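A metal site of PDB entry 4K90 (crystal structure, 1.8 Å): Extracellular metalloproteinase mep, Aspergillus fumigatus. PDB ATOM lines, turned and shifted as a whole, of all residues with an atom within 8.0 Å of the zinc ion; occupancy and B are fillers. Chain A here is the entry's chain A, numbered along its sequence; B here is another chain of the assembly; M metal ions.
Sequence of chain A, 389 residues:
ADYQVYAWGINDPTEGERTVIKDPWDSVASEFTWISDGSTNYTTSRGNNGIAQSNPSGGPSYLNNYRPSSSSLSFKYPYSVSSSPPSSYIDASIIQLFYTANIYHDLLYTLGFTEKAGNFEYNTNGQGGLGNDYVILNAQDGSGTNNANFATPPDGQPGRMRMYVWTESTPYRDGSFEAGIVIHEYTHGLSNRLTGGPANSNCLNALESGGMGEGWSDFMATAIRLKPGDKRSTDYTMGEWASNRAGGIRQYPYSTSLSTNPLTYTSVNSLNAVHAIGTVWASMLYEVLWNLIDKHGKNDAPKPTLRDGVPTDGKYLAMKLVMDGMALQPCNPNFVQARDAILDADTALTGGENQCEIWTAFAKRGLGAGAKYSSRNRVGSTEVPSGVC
Residues that only touch the zinc ion: His 275 (3.9 Å).
Of the 22 residues printed, 5 come within 4 Å of the zinc ion.
The nearest printed residue that does not touch the zinc ion is Ser 217 (4.6 Å).
The zinc ion is bound by OXT of Glu 215 of chain B, OE1 of Glu 214 of chain A, NE2 of His 188 and NE2 of His 184.
Slightly farther from the zinc ion lies the chain-end carboxylate (O) of Glu 215 of chain B (2.6 Å).
The chain-end carboxylate of Glu 215 of chain B lies close to a ring nitrogen (NE2) of His 275, 2.9 Å away.
The chain-end carboxylate of Glu 215 of chain B lies close to the side-chain carboxylate of Glu 185, 2.7 Å away.
ND2 of Asn 147 sits at hydrogen-bond distance from OE2 of Glu 215 of chain B, 3.3 Å away.
The side-chain carboxylate of Glu 214 of chain A lies close to a ring nitrogen (NE2) of His 275 (3.3 Å).
The side-chain hydroxyl (OG) of Ser 217 sits at hydrogen-bond distance from the backbone NH (N) of His 188 (3.4 Å).
The backbone carbonyl oxygen of His 184 is in hydrogen-bond range of the side-chain hydroxyl of Ser 217 (2.8 Å).
A ring nitrogen (ND1) of His 184 is in hydrogen-bond range of the side-chain carboxylate (OD1) of Asp 218, at 2.8 Å.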
ATOM      1  N   ASN A 147     -28.628  -8.727  16.421  1.00  0.00           N
ATOM      2  CA  ASN A 147     -29.139  -7.512  15.839  1.00  0.00           C
ATOM      3  C   ASN A 147     -29.626  -6.608  16.963  1.00  0.00           C
ATOM      4  O   ASN A 147     -29.396  -6.891  18.134  1.00  0.00           O
ATOM      5  CB  ASN A 147     -30.297  -7.852  14.886  1.00  0.00           C
ATOM      6  CG  ASN A 147     -30.260  -7.052  13.605  1.00  0.00           C
ATOM      7  OD1 ASN A 147     -30.104  -5.823  13.628  1.00  0.00           O
ATOM      8  ND2 ASN A 147     -30.426  -7.737  12.469  1.00  0.00           N
ATOM      9  N   ALA A 148     -30.300  -5.539  16.577  1.00  0.00           N
ATOM     10  CA  ALA A 148     -30.996  -4.639  17.500  1.00  0.00           C
ATOM     11  C   ALA A 148     -31.860  -3.751  16.623  1.00  0.00           C
ATOM     12  O   ALA A 148     -31.650  -3.655  15.395  1.00  0.00           O
ATOM     13  CB  ALA A 148     -30.023  -3.800  18.308  1.00  0.00           C
ATOM     14  N   ASN A 149     -32.852  -3.114  17.236  1.00  0.00           N
ATOM     15  CA  ASN A 149     -33.750  -2.274  16.461  1.00  0.00           C
ATOM     16  C   ASN A 149     -34.359  -1.165  17.294  1.00  0.00           C
ATOM     17  O   ASN A 149     -34.281  -1.189  18.529  1.00  0.00           O
ATOM     18  CB  ASN A 149     -34.799  -3.096  15.707  1.00  0.00           C
ATOM     19  CG  ASN A 149     -35.453  -4.138  16.567  1.00  0.00           C
ATOM     20  OD1 ASN A 149     -36.282  -3.819  17.420  1.00  0.00           O
ATOM     21  ND2 ASN A 149     -35.080  -5.405  16.345  1.00  0.00           N
ATOM     22  N   PHE A 150     -34.930  -0.173  16.608  1.00  0.00           N
ATOM     23  CA  PHE A 150     -35.429   1.026  17.267  1.00  0.00           C
ATOM     24  C   PHE A 150     -36.613   1.544  16.486  1.00  0.00           C
ATOM     25  O   PHE A 150     -36.542   1.714  15.257  1.00  0.00           O
ATOM     26  CB  PHE A 150     -34.334   2.121  17.380  1.00  0.00           C
ATOM     27  CG  PHE A 150     -34.710   3.261  18.313  1.00  0.00           C
ATOM     28  CD1 PHE A 150     -34.219   3.291  19.622  1.00  0.00           C
ATOM     29  CD2 PHE A 150     -35.557   4.297  17.887  1.00  0.00           C
ATOM     30  CE1 PHE A 150     -34.559   4.319  20.487  1.00  0.00           C
ATOM     31  CE2 PHE A 150     -35.933   5.329  18.758  1.00  0.00           C
ATOM     32  CZ  PHE A 150     -35.419   5.339  20.073  1.00  0.00           C
ATOM     33  N   ILE A 181     -23.717  -0.077  19.684  1.00  0.00           N
ATOM     34  CA  ILE A 181     -25.002  -0.566  19.197  1.00  0.00           C
ATOM     35  C   ILE A 181     -26.158   0.221  19.826  1.00  0.00           C
ATOM     36  O   ILE A 181     -27.120   0.584  19.131  1.00  0.00           O
ATOM     37  CB  ILE A 181     -25.172  -2.103  19.467  1.00  0.00           C
ATOM     38  CG1 ILE A 181     -24.068  -2.859  18.702  1.00  0.00           C
ATOM     39  CG2 ILE A 181     -26.565  -2.587  19.056  1.00  0.00           C
ATOM     40  CD1 ILE A 181     -24.036  -4.364  18.955  1.00  0.00           C
ATOM     41  N   HIS A 184     -26.074   3.504  18.118  1.00  0.00           N
ATOM     42  CA  HIS A 184     -26.644   3.313  16.784  1.00  0.00           C
ATOM     43  C   HIS A 184     -28.174   3.303  16.811  1.00  0.00           C
ATOM     44  O   HIS A 184     -28.814   4.022  16.020  1.00  0.00           O
ATOM     45  CB  HIS A 184     -26.115   2.032  16.113  1.00  0.00           C
ATOM     46  CG  HIS A 184     -26.681   1.780  14.745  1.00  0.00           C
ATOM     47  ND1 HIS A 184     -25.946   1.932  13.590  1.00  0.00           N
ATOM     48  CD2 HIS A 184     -27.927   1.398  14.360  1.00  0.00           C
ATOM     49  CE1 HIS A 184     -26.718   1.647  12.538  1.00  0.00           C
ATOM     50  NE2 HIS A 184     -27.913   1.322  12.984  1.00  0.00           N
ATOM     51  N   GLU A 185     -28.759   2.525  17.718  1.00  0.00           N
ATOM     52  CA  GLU A 185     -30.210   2.423  17.795  1.00  0.00           C
ATOM     53  C   GLU A 185     -30.858   3.759  18.179  1.00  0.00           C
ATOM     54  O   GLU A 185     -31.796   4.228  17.513  1.00  0.00           O
ATOM     55  CB  GLU A 185     -30.653   1.321  18.775  1.00  0.00           C
ATOM     56  CG  GLU A 185     -30.176  -0.088  18.418  1.00  0.00           C
ATOM     57  CD  GLU A 185     -30.375  -0.406  16.938  1.00  0.00           C
ATOM     58  OE1 GLU A 185     -31.468  -0.105  16.400  1.00  0.00           O
ATOM     59  OE2 GLU A 185     -29.458  -0.964  16.320  1.00  0.00           O
ATOM     60  N   THR A 187     -29.766   6.681  17.910  1.00  0.00           N
ATOM     61  CA  THR A 187     -29.574   7.699  16.858  1.00  0.00           C
ATOM     62  C   THR A 187     -30.684   7.617  15.785  1.00  0.00           C
ATOM     63  O   THR A 187     -31.029   8.646  15.195  1.00  0.00           O
ATOM     64  CB  THR A 187     -28.168   7.620  16.268  1.00  0.00           C
ATOM     65  OG1 THR A 187     -27.209   7.790  17.332  1.00  0.00           O
ATOM     66  CG2 THR A 187     -27.922   8.720  15.214  1.00  0.00           C
ATOM     67  N   HIS A 188     -31.250   6.433  15.550  1.00  0.00           N
ATOM     68  CA  HIS A 188     -32.432   6.333  14.675  1.00  0.00           C
ATOM     69  C   HIS A 188     -33.594   7.209  15.183  1.00  0.00           C
ATOM     70  O   HIS A 188     -34.319   7.828  14.402  1.00  0.00           O
ATOM     71  CB  HIS A 188     -32.902   4.874  14.489  1.00  0.00           C
ATOM     72  CG  HIS A 188     -32.064   4.096  13.519  1.00  0.00           C
ATOM     73  ND1 HIS A 188     -31.732   4.581  12.269  1.00  0.00           N
ATOM     74  CD2 HIS A 188     -31.485   2.878  13.620  1.00  0.00           C
ATOM     75  CE1 HIS A 188     -30.996   3.677  11.633  1.00  0.00           C
ATOM     76  NE2 HIS A 188     -30.838   2.633  12.433  1.00  0.00           N
ATOM     77  N   GLY A 210     -33.168   6.509   4.110  1.00  0.00           N
ATOM     78  CA  GLY A 210     -32.959   5.476   5.137  1.00  0.00           C
ATOM     79  C   GLY A 210     -31.509   5.031   5.177  1.00  0.00           C
ATOM     80  O   GLY A 210     -30.998   4.690   6.222  1.00  0.00           O
ATOM     81  N   GLY A 211     -30.851   5.021   4.015  1.00  0.00           N
ATOM     82  CA  GLY A 211     -29.401   4.771   3.960  1.00  0.00           C
ATOM     83  C   GLY A 211     -28.643   5.772   4.823  1.00  0.00           C
ATOM     84  O   GLY A 211     -27.830   5.395   5.681  1.00  0.00           O
ATOM     85  N   GLY A 213     -29.915   7.427   7.171  1.00  0.00           N
ATOM     86  CA  GLY A 213     -30.350   7.029   8.533  1.00  0.00           C
ATOM     87  C   GLY A 213     -29.359   6.053   9.176  1.00  0.00           C
ATOM     88  O   GLY A 213     -28.907   6.261  10.318  1.00  0.00           O
ATOM     89  N   GLU A 214     -28.971   5.033   8.421  1.00  0.00           N
ATOM     90  CA  GLU A 214     -27.994   4.056   8.919  1.00  0.00           C
ATOM     91  C   GLU A 214     -26.633   4.706   9.139  1.00  0.00           C
ATOM     92  O   GLU A 214     -25.990   4.470  10.166  1.00  0.00           O
ATOM     93  CB  GLU A 214     -27.900   2.856   7.944  1.00  0.00           C
ATOM     94  CG  GLU A 214     -29.190   2.059   7.830  1.00  0.00           C
ATOM     95  CD  GLU A 214     -29.751   1.616   9.184  1.00  0.00           C
ATOM     96  OE1 GLU A 214     -28.948   1.415  10.135  1.00  0.00           O
ATOM     97  OE2 GLU A 214     -30.985   1.485   9.306  1.00  0.00           O
ATOM     98  N   GLY A 215     -26.216   5.541   8.170  1.00  0.00           N
ATOM     99  CA  GLY A 215     -24.939   6.277   8.246  1.00  0.00           C
ATOM    100  C   GLY A 215     -24.834   7.183   9.475  1.00  0.00           C
ATOM    101  O   GLY A 215     -23.800   7.182  10.166  1.00  0.00           O
ATOM    102  N   TRP A 216     -25.874   7.986   9.735  1.00  0.00           N
ATOM    103  CA  TRP A 216     -25.873   8.851  10.936  1.00  0.00           C
ATOM    104  C   TRP A 216     -25.717   8.025  12.207  1.00  0.00           C
ATOM    105  O   TRP A 216     -24.991   8.427  13.117  1.00  0.00           O
ATOM    106  CB  TRP A 216     -27.138   9.703  11.030  1.00  0.00           C
ATOM    107  CG  TRP A 216     -27.141  10.914  10.102  1.00  0.00           C
ATOM    108  CD1 TRP A 216     -26.202  11.914  10.050  1.00  0.00           C
ATOM    109  CD2 TRP A 216     -28.158  11.270   9.146  1.00  0.00           C
ATOM    110  NE1 TRP A 216     -26.556  12.856   9.102  1.00  0.00           N
ATOM    111  CE2 TRP A 216     -27.741  12.484   8.521  1.00  0.00           C
ATOM    112  CE3 TRP A 216     -29.352  10.662   8.716  1.00  0.00           C
ATOM    113  CZ2 TRP A 216     -28.501  13.108   7.517  1.00  0.00           C
ATOM    114  CZ3 TRP A 216     -30.106  11.292   7.717  1.00  0.00           C
ATOM    115  CH2 TRP A 216     -29.679  12.496   7.131  1.00  0.00           C
ATOM    116  N   SER A 217     -26.406   6.881  12.260  1.00  0.00           N
ATOM    117  CA  SER A 217     -26.332   5.995  13.421  1.00  0.00           C
ATOM    118  C   SER A 217     -24.929   5.413  13.663  1.00  0.00           C
ATOM    119  O   SER A 217     -24.442   5.438  14.807  1.00  0.00           O
ATOM    120  CB  SER A 217     -27.379   4.882  13.311  1.00  0.00           C
ATOM    121  OG  SER A 217     -28.694   5.381  13.624  1.00  0.00           O
ATOM    122  N   ASP A 218     -24.274   4.906  12.610  1.00  0.00           N
ATOM    123  CA  ASP A 218     -22.871   4.452  12.716  1.00  0.00           C
ATOM    124  C   ASP A 218     -21.924   5.601  13.033  1.00  0.00           C
ATOM    125  O   ASP A 218     -20.941   5.439  13.800  1.00  0.00           O
ATOM    126  CB  ASP A 218     -22.406   3.821  11.401  1.00  0.00           C
ATOM    127  CG  ASP A 218     -22.888   2.390  11.208  1.00  0.00           C
ATOM    128  OD1 ASP A 218     -23.669   1.889  12.036  1.00  0.00           O
ATOM    129  OD2 ASP A 218     -22.493   1.766  10.199  1.00  0.00           O
ATOM    130  N   ARG A 250     -19.876  -4.018   8.811  1.00  0.00           N
ATOM    131  CA  ARG A 250     -19.979  -3.261   7.566  1.00  0.00           C
ATOM    132  C   ARG A 250     -18.932  -3.703   6.539  1.00  0.00           C
ATOM    133  O   ARG A 250     -17.974  -4.404   6.894  1.00  0.00           O
ATOM    134  CB  ARG A 250     -19.864  -1.736   7.803  1.00  0.00           C
ATOM    135  CG  ARG A 250     -20.814  -1.191   8.877  1.00  0.00           C
ATOM    136  CD  ARG A 250     -22.283  -1.474   8.612  1.00  0.00           C
ATOM    137  NE  ARG A 250     -23.087  -0.867   9.674  1.00  0.00           N
ATOM    138  CZ  ARG A 250     -24.216  -1.376  10.169  1.00  0.00           C
ATOM    139  NH1 ARG A 250     -24.733  -2.517   9.689  1.00  0.00           N
ATOM    140  NH2 ARG A 250     -24.838  -0.718  11.153  1.00  0.00           N
ATOM    141  N   VAL A 274     -30.304  -0.433   2.881  1.00  0.00           N
ATOM    142  CA  VAL A 274     -29.957   0.766   3.645  1.00  0.00           C
ATOM    143  C   VAL A 274     -28.662   0.683   4.445  1.00  0.00           C
ATOM    144  O   VAL A 274     -27.960   1.687   4.584  1.00  0.00           O
ATOM    145  CB  VAL A 274     -31.109   1.286   4.520  1.00  0.00           C
ATOM    146  CG1 VAL A 274     -32.275   1.752   3.632  1.00  0.00           C
ATOM    147  CG2 VAL A 274     -31.577   0.223   5.524  1.00  0.00           C
ATOM    148  N   HIS A 275     -28.323  -0.491   4.988  1.00  0.00           N
ATOM    149  CA  HIS A 275     -27.049  -0.587   5.750  1.00  0.00           C
ATOM    150  C   HIS A 275     -25.822  -0.353   4.887  1.00  0.00           C
ATOM    151  O   HIS A 275     -24.894   0.335   5.302  1.00  0.00           O
ATOM    152  CB  HIS A 275     -26.928  -1.897   6.550  1.00  0.00           C
ATOM    153  CG  HIS A 275     -27.946  -2.014   7.637  1.00  0.00           C
ATOM    154  ND1 HIS A 275     -29.037  -2.855   7.545  1.00  0.00           N
ATOM    155  CD2 HIS A 275     -28.064  -1.364   8.821  1.00  0.00           C
ATOM    156  CE1 HIS A 275     -29.765  -2.743   8.640  1.00  0.00           C
ATOM    157  NE2 HIS A 275     -29.204  -1.842   9.426  1.00  0.00           N
ATOM    158  N   ALA B 214     -36.479   0.678  12.599  1.00  0.00           N
ATOM    159  CA  ALA B 214     -35.217   0.564  11.883  1.00  0.00           C
ATOM    160  C   ALA B 214     -34.313  -0.408  12.640  1.00  0.00           C
ATOM    161  O   ALA B 214     -34.401  -0.516  13.877  1.00  0.00           O
ATOM    162  CB  ALA B 214     -34.550   1.930  11.805  1.00  0.00           C
ATOM    163  N   GLU B 215     -33.444  -1.086  11.908  1.00  0.00           N
ATOM    164  CA  GLU B 215     -32.362  -1.838  12.526  1.00  0.00           C
ATOM    165  C   GLU B 215     -31.181  -0.896  12.670  1.00  0.00           C
ATOM    166  O   GLU B 215     -30.973  -0.316  13.744  1.00  0.00           O
ATOM    167  CB  GLU B 215     -31.989  -3.067  11.703  1.00  0.00           C
ATOM    168  CG  GLU B 215     -33.095  -4.109  11.691  1.00  0.00           C
ATOM    169  CD  GLU B 215     -32.661  -5.427  11.102  1.00  0.00           C
ATOM    170  OE1 GLU B 215     -31.697  -5.450  10.312  1.00  0.00           O
ATOM    171  OE2 GLU B 215     -33.307  -6.454  11.452  1.00  0.00           O
ATOM    172  OXT GLU B 215     -30.442  -0.649  11.711  1.00  0.00           O
HETATM  173 ZN    ZN M   1     -29.652   1.115  11.948  1.00  0.00          ZN
